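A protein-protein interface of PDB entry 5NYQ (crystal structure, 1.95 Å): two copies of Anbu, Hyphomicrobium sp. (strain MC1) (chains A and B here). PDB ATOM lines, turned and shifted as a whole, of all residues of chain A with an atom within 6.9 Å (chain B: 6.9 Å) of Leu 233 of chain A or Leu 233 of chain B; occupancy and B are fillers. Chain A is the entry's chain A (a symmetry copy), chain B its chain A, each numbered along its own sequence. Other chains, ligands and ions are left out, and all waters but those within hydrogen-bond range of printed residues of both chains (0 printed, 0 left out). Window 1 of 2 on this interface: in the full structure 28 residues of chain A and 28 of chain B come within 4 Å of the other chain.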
ATOM      1  N   PRO A 160     -11.218 -18.157   0.303  1.00  0.00           N
ATOM      2  CA  PRO A 160     -12.149 -17.439  -0.582  1.00  0.00           C
ATOM      3  C   PRO A 160     -13.494 -18.134  -0.798  1.00  0.00           C
ATOM      4  O   PRO A 160     -14.526 -17.467  -0.795  1.00  0.00           O
ATOM      5  CB  PRO A 160     -11.383 -17.354  -1.908  1.00  0.00           C
ATOM      6  CG  PRO A 160      -9.955 -17.372  -1.508  1.00  0.00           C
ATOM      7  CD  PRO A 160      -9.892 -18.307  -0.336  1.00  0.00           C
ATOM      8  N   ILE A 161     -13.470 -19.454  -0.972  1.00  0.00           N
ATOM      9  CA  ILE A 161     -14.692 -20.231  -1.180  1.00  0.00           C
ATOM     10  C   ILE A 161     -15.566 -20.201   0.078  1.00  0.00           C
ATOM     11  O   ILE A 161     -16.780 -20.026  -0.026  1.00  0.00           O
ATOM     12  CB  ILE A 161     -14.386 -21.679  -1.659  1.00  0.00           C
ATOM     13  CG1 ILE A 161     -14.114 -21.701  -3.171  1.00  0.00           C
ATOM     14  CG2 ILE A 161     -15.558 -22.628  -1.410  1.00  0.00           C
ATOM     15  CD1 ILE A 161     -13.156 -20.644  -3.693  1.00  0.00           C
ATOM     16  N   ARG A 164     -17.246 -16.775   0.551  1.00  0.00           N
ATOM     17  CA  ARG A 164     -18.294 -16.523  -0.444  1.00  0.00           C
ATOM     18  C   ARG A 164     -19.525 -17.433  -0.309  1.00  0.00           C
ATOM     19  O   ARG A 164     -20.637 -17.014  -0.643  1.00  0.00           O
ATOM     20  CB  ARG A 164     -17.708 -16.660  -1.858  1.00  0.00           C
ATOM     21  CG  ARG A 164     -16.666 -15.600  -2.218  1.00  0.00           C
ATOM     22  CD  ARG A 164     -15.909 -15.989  -3.484  1.00  0.00           C
ATOM     23  NE  ARG A 164     -14.848 -15.049  -3.865  1.00  0.00           N
ATOM     24  CZ  ARG A 164     -14.996 -13.959  -4.628  1.00  0.00           C
ATOM     25  NH1 ARG A 164     -16.182 -13.599  -5.127  1.00  0.00           N
ATOM     26  NH2 ARG A 164     -13.932 -13.206  -4.901  1.00  0.00           N
ATOM     27  N   VAL A 165     -19.324 -18.663   0.170  1.00  0.00           N
ATOM     28  CA  VAL A 165     -20.382 -19.696   0.189  1.00  0.00           C
ATOM     29  C   VAL A 165     -20.945 -20.000   1.592  1.00  0.00           C
ATOM     30  O   VAL A 165     -22.138 -20.287   1.720  1.00  0.00           O
ATOM     31  CB  VAL A 165     -19.882 -20.992  -0.500  1.00  0.00           C
ATOM     32  CG1 VAL A 165     -20.939 -22.093  -0.481  1.00  0.00           C
ATOM     33  CG2 VAL A 165     -19.470 -20.694  -1.938  1.00  0.00           C
ATOM     34  N   SER A 226     -15.647 -34.397  -4.590  1.00  0.00           N
ATOM     35  CA  SER A 226     -14.569 -33.563  -5.132  1.00  0.00           C
ATOM     36  C   SER A 226     -14.604 -33.446  -6.656  1.00  0.00           C
ATOM     37  O   SER A 226     -14.404 -32.359  -7.188  1.00  0.00           O
ATOM     38  CB  SER A 226     -13.201 -34.092  -4.697  1.00  0.00           C
ATOM     39  OG  SER A 226     -12.169 -33.237  -5.157  1.00  0.00           O
ATOM     40  N   ALA A 228     -17.313 -33.852  -8.558  1.00  0.00           N
ATOM     41  CA  ALA A 228     -18.504 -33.049  -8.859  1.00  0.00           C
ATOM     42  C   ALA A 228     -18.243 -31.558  -8.635  1.00  0.00           C
ATOM     43  O   ALA A 228     -18.691 -30.731  -9.428  1.00  0.00           O
ATOM     44  CB  ALA A 228     -19.694 -33.512  -8.025  1.00  0.00           C
ATOM     45  N   TRP A 229     -17.520 -31.228  -7.560  1.00  0.00           N
ATOM     46  CA  TRP A 229     -17.139 -29.843  -7.262  1.00  0.00           C
ATOM     47  C   TRP A 229     -16.299 -29.223  -8.387  1.00  0.00           C
ATOM     48  O   TRP A 229     -16.585 -28.111  -8.831  1.00  0.00           O
ATOM     49  CB  TRP A 229     -16.398 -29.781  -5.921  1.00  0.00           C
ATOM     50  CG  TRP A 229     -15.960 -28.412  -5.464  1.00  0.00           C
ATOM     51  CD1 TRP A 229     -14.700 -28.049  -5.074  1.00  0.00           C
ATOM     52  CD2 TRP A 229     -16.775 -27.239  -5.322  1.00  0.00           C
ATOM     53  NE1 TRP A 229     -14.679 -26.727  -4.703  1.00  0.00           N
ATOM     54  CE2 TRP A 229     -15.937 -26.205  -4.844  1.00  0.00           C
ATOM     55  CE3 TRP A 229     -18.129 -26.959  -5.552  1.00  0.00           C
ATOM     56  CZ2 TRP A 229     -16.411 -24.909  -4.590  1.00  0.00           C
ATOM     57  CZ3 TRP A 229     -18.598 -25.666  -5.309  1.00  0.00           C
ATOM     58  CH2 TRP A 229     -17.739 -24.660  -4.831  1.00  0.00           C
ATOM     59  N   SER A 230     -15.285 -29.951  -8.854  1.00  0.00           N
ATOM     60  CA  SER A 230     -14.471 -29.509 -10.000  1.00  0.00           C
ATOM     61  C   SER A 230     -15.314 -29.245 -11.243  1.00  0.00           C
ATOM     62  O   SER A 230     -15.155 -28.209 -11.891  1.00  0.00           O
ATOM     63  CB  SER A 230     -13.390 -30.537 -10.337  1.00  0.00           C
ATOM     64  OG  SER A 230     -12.434 -30.601  -9.305  1.00  0.00           O
ATOM     65  N   ASP A 231     -16.212 -30.179 -11.559  1.00  0.00           N
ATOM     66  CA  ASP A 231     -17.136 -30.020 -12.688  1.00  0.00           C
ATOM     67  C   ASP A 231     -18.013 -28.780 -12.512  1.00  0.00           C
ATOM     68  O   ASP A 231     -18.191 -28.009 -13.452  1.00  0.00           O
ATOM     69  CB  ASP A 231     -18.023 -31.266 -12.865  1.00  0.00           C
ATOM     70  CG  ASP A 231     -17.243 -32.501 -13.315  1.00  0.00           C
ATOM     71  OD1 ASP A 231     -16.038 -32.395 -13.619  1.00  0.00           O
ATOM     72  OD2 ASP A 231     -17.845 -33.596 -13.366  1.00  0.00           O
ATOM     73  N   ALA A 232     -18.539 -28.593 -11.302  1.00  0.00           N
ATOM     74  CA  ALA A 232     -19.378 -27.436 -10.978  1.00  0.00           C
ATOM     75  C   ALA A 232     -18.617 -26.106 -11.042  1.00  0.00           C
ATOM     76  O   ALA A 232     -19.174 -25.097 -11.477  1.00  0.00           O
ATOM     77  CB  ALA A 232     -20.010 -27.615  -9.604  1.00  0.00           C
ATOM     78  N   LEU A 233     -17.362 -26.108 -10.596  1.00  0.00           N
ATOM     79  CA  LEU A 233     -16.501 -24.917 -10.679  1.00  0.00           C
ATOM     80  C   LEU A 233     -16.240 -24.479 -12.115  1.00  0.00           C
ATOM     81  O   LEU A 233     -16.303 -23.280 -12.426  1.00  0.00           O
ATOM     82  CB  LEU A 233     -15.168 -25.159  -9.970  1.00  0.00           C
ATOM     83  CG  LEU A 233     -15.227 -25.118  -8.442  1.00  0.00           C
ATOM     84  CD1 LEU A 233     -13.927 -25.640  -7.863  1.00  0.00           C
ATOM     85  CD2 LEU A 233     -15.514 -23.708  -7.944  1.00  0.00           C
ATOM     86  N   ARG A 234     -15.948 -25.451 -12.976  1.00  0.00           N
ATOM     87  CA  ARG A 234     -15.731 -25.191 -14.397  1.00  0.00           C
ATOM     88  C   ARG A 234     -16.985 -24.618 -15.044  1.00  0.00           C
ATOM     89  O   ARG A 234     -16.894 -23.680 -15.832  1.00  0.00           O
ATOM     90  CB  ARG A 234     -15.282 -26.458 -15.126  1.00  0.00           C
ATOM     91  CG  ARG A 234     -13.893 -26.922 -14.723  1.00  0.00           C
ATOM     92  CD  ARG A 234     -13.385 -28.071 -15.583  1.00  0.00           C
ATOM     93  NE  ARG A 234     -12.981 -29.212 -14.754  1.00  0.00           N
ATOM     94  CZ  ARG A 234     -13.643 -30.369 -14.620  1.00  0.00           C
ATOM     95  NH1 ARG A 234     -14.784 -30.617 -15.270  1.00  0.00           N
ATOM     96  NH2 ARG A 234     -13.145 -31.310 -13.819  1.00  0.00           N
ATOM     97  N   GLN A 235     -18.146 -25.173 -14.693  1.00  0.00           N
ATOM     98  CA  GLN A 235     -19.429 -24.634 -15.150  1.00  0.00           C
ATOM     99  C   GLN A 235     -19.695 -23.230 -14.598  1.00  0.00           C
ATOM    100  O   GLN A 235     -20.165 -22.364 -15.329  1.00  0.00           O
ATOM    101  CB  GLN A 235     -20.585 -25.577 -14.788  1.00  0.00           C
ATOM    102  CG  GLN A 235     -20.553 -26.885 -15.556  1.00  0.00           C
ATOM    103  CD  GLN A 235     -21.649 -27.851 -15.139  1.00  0.00           C
ATOM    104  OE1 GLN A 235     -22.823 -27.645 -15.451  1.00  0.00           O
ATOM    105  NE2 GLN A 235     -21.267 -28.923 -14.452  1.00  0.00           N
ATOM    106  N   ALA A 236     -19.390 -23.008 -13.319  1.00  0.00           N
ATOM    107  CA  ALA A 236     -19.534 -21.676 -12.705  1.00  0.00           C
ATOM    108  C   ALA A 236     -18.651 -20.635 -13.405  1.00  0.00           C
ATOM    109  O   ALA A 236     -19.100 -19.514 -13.693  1.00  0.00           O
ATOM    110  CB  ALA A 236     -19.199 -21.728 -11.221  1.00  0.00           C
ATOM    111  N   PHE A 237     -17.406 -21.011 -13.696  1.00  0.00           N
ATOM    112  CA  PHE A 237     -16.508 -20.108 -14.406  1.00  0.00           C
ATOM    113  C   PHE A 237     -16.981 -19.851 -15.842  1.00  0.00           C
ATOM    114  O   PHE A 237     -16.914 -18.717 -16.318  1.00  0.00           O
ATOM    115  CB  PHE A 237     -15.063 -20.611 -14.405  1.00  0.00           C
ATOM    116  CG  PHE A 237     -14.109 -19.629 -15.008  1.00  0.00           C
ATOM    117  CD1 PHE A 237     -13.809 -18.448 -14.340  1.00  0.00           C
ATOM    118  CD2 PHE A 237     -13.564 -19.845 -16.269  1.00  0.00           C
ATOM    119  CE1 PHE A 237     -12.951 -17.514 -14.905  1.00  0.00           C
ATOM    120  CE2 PHE A 237     -12.711 -18.915 -16.839  1.00  0.00           C
ATOM    121  CZ  PHE A 237     -12.404 -17.750 -16.153  1.00  0.00           C
ATOM    122  N   SER A 238     -17.462 -20.894 -16.518  1.00  0.00           N
ATOM    123  CA  SER A 238     -18.044 -20.743 -17.860  1.00  0.00           C
ATOM    124  C   SER A 238     -19.190 -19.734 -17.920  1.00  0.00           C
ATOM    125  O   SER A 238     -19.321 -19.018 -18.907  1.00  0.00           O
ATOM    126  CB  SER A 238     -18.524 -22.088 -18.415  1.00  0.00           C
ATOM    127  OG  SER A 238     -17.423 -22.871 -18.828  1.00  0.00           O
ATOM    128  N   LYS A 239     -20.013 -19.679 -16.874  1.00  0.00           N
ATOM    129  CA  LYS A 239     -21.113 -18.706 -16.808  1.00  0.00           C
ATOM    130  C   LYS A 239     -20.564 -17.281 -16.723  1.00  0.00           C
ATOM    131  O   LYS A 239     -20.865 -16.435 -17.569  1.00  0.00           O
ATOM    132  CB  LYS A 239     -22.010 -18.972 -15.594  1.00  0.00           C
ATOM    133  CG  LYS A 239     -22.759 -20.296 -15.613  1.00  0.00           C
ATOM    134  CD  LYS A 239     -24.064 -20.229 -16.393  1.00  0.00           C
ATOM    135  CE  LYS A 239     -24.948 -21.427 -16.074  1.00  0.00           C
ATOM    136  NZ  LYS A 239     -26.137 -21.501 -16.968  1.00  0.00           N
ATOM    137  N   ILE A 240     -19.731 -17.046 -15.712  1.00  0.00           N
ATOM    138  CA  ILE A 240     -19.293 -15.694 -15.344  1.00  0.00           C
ATOM    139  C   ILE A 240     -18.214 -15.076 -16.239  1.00  0.00           C
ATOM    140  O   ILE A 240     -17.927 -13.881 -16.113  1.00  0.00           O
ATOM    141  CB  ILE A 240     -18.836 -15.619 -13.864  1.00  0.00           C
ATOM    142  CG1 ILE A 240     -17.553 -16.432 -13.615  1.00  0.00           C
ATOM    143  CG2 ILE A 240     -19.966 -16.061 -12.938  1.00  0.00           C
ATOM    144  CD1 ILE A 240     -16.296 -15.603 -13.502  1.00  0.00           C
ATOM    145  N   PRO B 160      -6.628 -24.085  -5.144  1.00  0.00           N
ATOM    146  CA  PRO B 160      -7.602 -25.124  -5.515  1.00  0.00           C
ATOM    147  C   PRO B 160      -8.451 -24.799  -6.743  1.00  0.00           C
ATOM    148  O   PRO B 160      -8.675 -25.678  -7.573  1.00  0.00           O
ATOM    149  CB  PRO B 160      -8.496 -25.230  -4.272  1.00  0.00           C
ATOM    150  CG  PRO B 160      -7.615 -24.823  -3.151  1.00  0.00           C
ATOM    151  CD  PRO B 160      -6.752 -23.731  -3.714  1.00  0.00           C
ATOM    152  N   ILE B 161      -8.904 -23.552  -6.853  1.00  0.00           N
ATOM    153  CA  ILE B 161      -9.720 -23.119  -7.987  1.00  0.00           C
ATOM    154  C   ILE B 161      -8.901 -23.158  -9.281  1.00  0.00           C
ATOM    155  O   ILE B 161      -9.399 -23.622 -10.305  1.00  0.00           O
ATOM    156  CB  ILE B 161     -10.373 -21.729  -7.738  1.00  0.00           C
ATOM    157  CG1 ILE B 161     -11.640 -21.875  -6.881  1.00  0.00           C
ATOM    158  CG2 ILE B 161     -10.798 -21.050  -9.038  1.00  0.00           C
ATOM    159  CD1 ILE B 161     -11.514 -22.749  -5.645  1.00  0.00           C
ATOM    160  N   ARG B 164      -8.301 -26.766 -10.465  1.00  0.00           N
ATOM    161  CA  ARG B 164      -9.524 -27.402 -10.967  1.00  0.00           C
ATOM    162  C   ARG B 164     -10.064 -26.791 -12.270  1.00  0.00           C
ATOM    163  O   ARG B 164     -10.678 -27.500 -13.072  1.00  0.00           O
ATOM    164  CB  ARG B 164     -10.614 -27.350  -9.885  1.00  0.00           C
ATOM    165  CG  ARG B 164     -10.311 -28.183  -8.639  1.00  0.00           C
ATOM    166  CD  ARG B 164     -11.263 -27.827  -7.502  1.00  0.00           C
ATOM    167  NE  ARG B 164     -11.000 -28.543  -6.249  1.00  0.00           N
ATOM    168  CZ  ARG B 164     -11.491 -29.741  -5.906  1.00  0.00           C
ATOM    169  NH1 ARG B 164     -12.293 -30.436  -6.717  1.00  0.00           N
ATOM    170  NH2 ARG B 164     -11.172 -30.260  -4.722  1.00  0.00           N
ATOM    171  N   VAL B 165      -9.843 -25.489 -12.470  1.00  0.00           N
ATOM    172  CA  VAL B 165     -10.454 -24.738 -13.589  1.00  0.00           C
ATOM    173  C   VAL B 165      -9.466 -24.362 -14.712  1.00  0.00           C
ATOM    174  O   VAL B 165      -9.856 -24.343 -15.883  1.00  0.00           O
ATOM    175  CB  VAL B 165     -11.189 -23.481 -13.055  1.00  0.00           C
ATOM    176  CG1 VAL B 165     -11.815 -22.665 -14.183  1.00  0.00           C
ATOM    177  CG2 VAL B 165     -12.265 -23.892 -12.054  1.00  0.00           C
ATOM    178  N   SER B 226     -16.412 -10.244  -9.616  1.00  0.00           N
ATOM    179  CA  SER B 226     -16.312 -10.878  -8.297  1.00  0.00           C
ATOM    180  C   SER B 226     -17.671 -11.231  -7.692  1.00  0.00           C
ATOM    181  O   SER B 226     -17.826 -12.310  -7.130  1.00  0.00           O
ATOM    182  CB  SER B 226     -15.540  -9.989  -7.322  1.00  0.00           C
ATOM    183  OG  SER B 226     -15.378 -10.642  -6.076  1.00  0.00           O
ATOM    184  N   ALA B 228     -20.474 -11.755  -9.421  1.00  0.00           N
ATOM    185  CA  ALA B 228     -20.997 -12.847 -10.250  1.00  0.00           C
ATOM    186  C   ALA B 228     -20.356 -14.187  -9.880  1.00  0.00           C
ATOM    187  O   ALA B 228     -21.044 -15.205  -9.835  1.00  0.00           O
ATOM    188  CB  ALA B 228     -20.790 -12.550 -11.732  1.00  0.00           C
ATOM    189  N   TRP B 229     -19.046 -14.173  -9.614  1.00  0.00           N
ATOM    190  CA  TRP B 229     -18.317 -15.371  -9.182  1.00  0.00           C
ATOM    191  C   TRP B 229     -18.879 -15.944  -7.873  1.00  0.00           C
ATOM    192  O   TRP B 229     -19.128 -17.146  -7.781  1.00  0.00           O
ATOM    193  CB  TRP B 229     -16.822 -15.056  -9.049  1.00  0.00           C
ATOM    194  CG  TRP B 229     -15.934 -16.201  -8.632  1.00  0.00           C
ATOM    195  CD1 TRP B 229     -15.035 -16.199  -7.600  1.00  0.00           C
ATOM    196  CD2 TRP B 229     -15.834 -17.494  -9.246  1.00  0.00           C
ATOM    197  NE1 TRP B 229     -14.388 -17.408  -7.532  1.00  0.00           N
ATOM    198  CE2 TRP B 229     -14.858 -18.222  -8.528  1.00  0.00           C
ATOM    199  CE3 TRP B 229     -16.475 -18.111 -10.329  1.00  0.00           C
ATOM    200  CZ2 TRP B 229     -14.503 -19.538  -8.862  1.00  0.00           C
ATOM    201  CZ3 TRP B 229     -16.129 -19.425 -10.655  1.00  0.00           C
ATOM    202  CH2 TRP B 229     -15.151 -20.121  -9.922  1.00  0.00           C
ATOM    203  N   SER B 230     -19.095 -15.081  -6.881  1.00  0.00           N
ATOM    204  CA  SER B 230     -19.727 -15.492  -5.614  1.00  0.00           C
ATOM    205  C   SER B 230     -21.095 -16.130  -5.828  1.00  0.00           C
ATOM    206  O   SER B 230     -21.381 -17.187  -5.265  1.00  0.00           O
ATOM    207  CB  SER B 230     -19.870 -14.306  -4.659  1.00  0.00           C
ATOM    208  OG  SER B 230     -18.604 -13.867  -4.228  1.00  0.00           O
ATOM    209  N   ASP B 231     -21.925 -15.488  -6.651  1.00  0.00           N
ATOM    210  CA  ASP B 231     -23.245 -16.025  -7.001  1.00  0.00           C
ATOM    211  C   ASP B 231     -23.123 -17.393  -7.673  1.00  0.00           C
ATOM    212  O   ASP B 231     -23.857 -18.318  -7.335  1.00  0.00           O
ATOM    213  CB  ASP B 231     -24.018 -15.059  -7.918  1.00  0.00           C
ATOM    214  CG  ASP B 231     -24.422 -13.761  -7.220  1.00  0.00           C
ATOM    215  OD1 ASP B 231     -24.229 -13.631  -5.995  1.00  0.00           O
ATOM    216  OD2 ASP B 231     -24.943 -12.856  -7.908  1.00  0.00           O
ATOM    217  N   ALA B 232     -22.183 -17.509  -8.611  1.00  0.00           N
ATOM    218  CA  ALA B 232     -21.932 -18.766  -9.323  1.00  0.00           C
ATOM    219  C   ALA B 232     -21.403 -19.879  -8.409  1.00  0.00           C
ATOM    220  O   ALA B 232     -21.767 -21.043  -8.580  1.00  0.00           O
ATOM    221  CB  ALA B 232     -20.968 -18.531 -10.479  1.00  0.00           C
ATOM    222  N   LEU B 233     -20.541 -19.519  -7.460  1.00  0.00           N
ATOM    223  CA  LEU B 233     -20.024 -20.478  -6.469  1.00  0.00           C
ATOM    224  C   LEU B 233     -21.120 -21.056  -5.584  1.00  0.00           C
ATOM    225  O   LEU B 233     -21.147 -22.271  -5.332  1.00  0.00           O
ATOM    226  CB  LEU B 233     -18.952 -19.830  -5.593  1.00  0.00           C
ATOM    227  CG  LEU B 233     -17.587 -19.650  -6.261  1.00  0.00           C
ATOM    228  CD1 LEU B 233     -16.708 -18.760  -5.405  1.00  0.00           C
ATOM    229  CD2 LEU B 233     -16.918 -20.996  -6.507  1.00  0.00           C
ATOM    230  N   ARG B 234     -22.014 -20.186  -5.119  1.00  0.00           N
ATOM    231  CA  ARG B 234     -23.154 -20.601  -4.306  1.00  0.00           C
ATOM    232  C   ARG B 234     -24.066 -21.540  -5.086  1.00  0.00           C
ATOM    233  O   ARG B 234     -24.526 -22.540  -4.540  1.00  0.00           O
ATOM    234  CB  ARG B 234     -23.938 -19.391  -3.797  1.00  0.00           C
ATOM    235  CG  ARG B 234     -23.172 -18.564  -2.781  1.00  0.00           C
ATOM    236  CD  ARG B 234     -24.025 -17.473  -2.149  1.00  0.00           C
ATOM    237  NE  ARG B 234     -23.393 -16.157  -2.295  1.00  0.00           N
ATOM    238  CZ  ARG B 234     -23.783 -15.177  -3.121  1.00  0.00           C
ATOM    239  NH1 ARG B 234     -24.846 -15.301  -3.923  1.00  0.00           N
ATOM    240  NH2 ARG B 234     -23.095 -14.036  -3.141  1.00  0.00           N
ATOM    241  N   GLN B 235     -24.304 -21.221  -6.359  1.00  0.00           N
ATOM    242  CA  GLN B 235     -25.063 -22.106  -7.247  1.00  0.00           C
ATOM    243  C   GLN B 235     -24.339 -23.432  -7.498  1.00  0.00           C
ATOM    244  O   GLN B 235     -24.970 -24.484  -7.492  1.00  0.00           O
ATOM    245  CB  GLN B 235     -25.379 -21.410  -8.579  1.00  0.00           C
ATOM    246  CG  GLN B 235     -26.362 -20.263  -8.437  1.00  0.00           C
ATOM    247  CD  GLN B 235     -26.611 -19.524  -9.741  1.00  0.00           C
ATOM    248  OE1 GLN B 235     -27.276 -20.040 -10.640  1.00  0.00           O
ATOM    249  NE2 GLN B 235     -26.099 -18.301  -9.839  1.00  0.00           N
ATOM    250  N   ALA B 236     -23.024 -23.380  -7.708  1.00  0.00           N
ATOM    251  CA  ALA B 236     -22.215 -24.601  -7.885  1.00  0.00           C
ATOM    252  C   ALA B 236     -22.282 -25.503  -6.647  1.00  0.00           C
ATOM    253  O   ALA B 236     -22.447 -26.728  -6.764  1.00  0.00           O
ATOM    254  CB  ALA B 236     -20.769 -24.247  -8.195  1.00  0.00           C
ATOM    255  N   PHE B 237     -22.174 -24.899  -5.465  1.00  0.00           N
ATOM    256  CA  PHE B 237     -22.275 -25.668  -4.230  1.00  0.00           C
ATOM    257  C   PHE B 237     -23.682 -26.242  -4.033  1.00  0.00           C
ATOM    258  O   PHE B 237     -23.826 -27.389  -3.606  1.00  0.00           O
ATOM    259  CB  PHE B 237     -21.859 -24.851  -3.005  1.00  0.00           C
ATOM    260  CG  PHE B 237     -21.825 -25.666  -1.750  1.00  0.00           C
ATOM    261  CD1 PHE B 237     -20.839 -26.630  -1.572  1.00  0.00           C
ATOM    262  CD2 PHE B 237     -22.810 -25.524  -0.780  1.00  0.00           C
ATOM    263  CE1 PHE B 237     -20.819 -27.415  -0.427  1.00  0.00           C
ATOM    264  CE2 PHE B 237     -22.796 -26.307   0.362  1.00  0.00           C
ATOM    265  CZ  PHE B 237     -21.796 -27.251   0.537  1.00  0.00           C
ATOM    266  N   SER B 238     -24.709 -25.454  -4.350  1.00  0.00           N
ATOM    267  CA  SER B 238     -26.097 -25.937  -4.306  1.00  0.00           C
ATOM    268  C   SER B 238     -26.339 -27.181  -5.160  1.00  0.00           C
ATOM    269  O   SER B 238     -27.112 -28.049  -4.768  1.00  0.00           O
ATOM    270  CB  SER B 238     -27.084 -24.840  -4.717  1.00  0.00           C
ATOM    271  OG  SER B 238     -27.232 -23.895  -3.677  1.00  0.00           O
ATOM    272  N   LYS B 239     -25.687 -27.264  -6.319  1.00  0.00           N
ATOM    273  CA  LYS B 239     -25.807 -28.443  -7.189  1.00  0.00           C
ATOM    274  C   LYS B 239     -25.200 -29.672  -6.512  1.00  0.00           C
ATOM    275  O   LYS B 239     -25.878 -30.684  -6.310  1.00  0.00           O
ATOM    276  CB  LYS B 239     -25.104 -28.210  -8.531  1.00  0.00           C
ATOM    277  CG  LYS B 239     -25.701 -27.113  -9.400  1.00  0.00           C
ATOM    278  CD  LYS B 239     -26.870 -27.597 -10.248  1.00  0.00           C
ATOM    279  CE  LYS B 239     -27.184 -26.601 -11.356  1.00  0.00           C
ATOM    280  NZ  LYS B 239     -28.442 -26.940 -12.076  1.00  0.00           N
ATOM    281  N   ILE B 240     -23.929 -29.553  -6.136  1.00  0.00           N
ATOM    282  CA  ILE B 240     -23.124 -30.695  -5.686  1.00  0.00           C
ATOM    283  C   ILE B 240     -23.391 -31.175  -4.256  1.00  0.00           C
ATOM    284  O   ILE B 240     -22.896 -32.238  -3.867  1.00  0.00           O
ATOM    285  CB  ILE B 240     -21.605 -30.436  -5.865  1.00  0.00           C
ATOM    286  CG1 ILE B 240     -21.097 -29.321  -4.934  1.00  0.00           C
ATOM    287  CG2 ILE B 240     -21.289 -30.131  -7.326  1.00  0.00           C
ATOM    288  CD1 ILE B 240     -20.342 -29.810  -3.721  1.00  0.00           C
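Of chain B, only Arg 164, Val 165 and Leu 233 come within 4 Å of Leu 233 of chain A.
Of chain A, only Arg 164, Val 165 and Leu 233 come within 4 Å of Leu 233 of chain B.
Of the printed residues of chain A, Ile 161 of chain B touches Ile 161 (3.3 Å).
Of the printed residues of chain B, Arg 234 of chain A touches Arg 164 (3.3 Å).
Of the printed residues of chain A, Ala 228 of chain B touches Ile 240 (3.4 Å).
Printed residues of chain B within 4 Å of Ile 240 of chain A: Ala 228, Trp 229 and Ala 232.
Gln 235 of chain B touches none of the printed residues of chain A.
Lys 239 of chain B touches none of the printed residues of chain A.
The guanidinium group of Arg 234 of chain A lies within hydrogen-bond range of the backbone carbonyl oxygen of Arg 164 of chain B.
The backbone carbonyl oxygen (O) of Ser 226 of chain A is in hydrogen-bond range of the guanidinium group (NH1) of Arg 164 of chain B (2.9 Å).
O of Ser 226 of chain B is in hydrogen-bond range of NH1 of Arg 164 of chain A (2.9 Å).
The side-chain hydroxyl of Ser 230 of chain B sits at hydrogen-bond distance from the guanidinium group of Arg 164 of chain A (2.6 Å).
OG of Ser 230 of chain A is in hydrogen-bond range of NH1 of Arg 164 of chain B, 2.6 Å away.
The backbone carbonyl oxygen of Arg 164 of chain A sits at hydrogen-bond distance from the guanidinium group of Arg 234 of chain B (3.3 Å).
CZ of Arg 164 of chain A touches CD1 of Trp 229 of chain B (3.7 Å).
CZ of Arg 164 of chain B touches CD1 of Trp 229 of chain A, at 3.7 Å.
Ala 236 of chain B touches Trp 229 of chain A.
Trp 229 of chain A touches Phe 237 of chain B (CZ3 to N, 3.7 Å).
Ala 232 of chain A touches Ile 240 of chain B.
Leu 233 of chain A touches Arg 164 of chain B.
Ala 236 of chain A touches Ala 232 of chain B (CB to CB, 3.7 Å).
CG2 of Ile 240 of chain A touches O of Ala 228 of chain B (3.4 Å).
Ile 240 of chain A touches Trp 229 of chain B (CG1 to CE3, 3.8 Å).
Ala 232 of chain B touches Ile 240 of chain A.
O of Ser 226 of chain A is in hydrogen-bond range of OG of Ser 230 of chain A.
The side-chain hydroxyl (OG) of Ser 238 of chain B sits at hydrogen-bond distance from the backbone carbonyl oxygen (O) of Arg 234 of chain B (3.1 Å).
The side-chain hydroxyl (OG) of Ser 238 of chain A is in hydrogen-bond range of the backbone carbonyl oxygen (O) of Arg 234 of chain A, 3.1 Å away.
The backbone carbonyl oxygen (O) of Ser 226 of chain B sits at hydrogen-bond distance from the side-chain hydroxyl (OG) of Ser 230 of chain B (3.4 Å).
NH1 of Arg 234 of chain A lies within salt-bridge range of OD1 of Asp 231 of chain A.
NH1 of Arg 234 of chain B lies within salt-bridge range of OD1 of Asp 231 of chain B (2.7 Å).
Ile 161 of chain A touches its own counterpart, Ile 161 of chain B.
Arg 164 of chain A touches Arg 234 of chain B, and with the chains exchanged Arg 234 of chain A touches Arg 164 of chain B.
Trp 229 of chain A touches Phe 237 of chain B, and with the chains exchanged Phe 237 of chain A touches Trp 229 of chain B.
Ala 232 of chain A touches Ile 240 of chain B, and with the chains exchanged Ile 240 of chain A touches Ala 232 of chain B.
Positions printed for both chains: 160, 161, 164, 165, 226, 228, 229, 230, 231, 232, 233, 234, 235, 236, 237, 238, 239 and 240.
Of the 28 pairs that touch across the chains among the printed residues, 28 have their exchanged pair printed and touching as well.
Hydrophobic or aromatic side chains of chain B within 4 Å of the printed part of chain A: Ile 161, Val 165, Ala 228, Trp 229, Ala 232, Leu 233, Ala 236, Phe 237 and Ile 240.
Of the 18 printed residues of chain A, 13 touch a printed residue of chain B.
Among the printed residues, 28 pairs touch across the chains.
Among the printed residues, no Asp or Glu carboxylate lies within 4 Å of a Lys or Arg side-chain nitrogen of the other chain.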
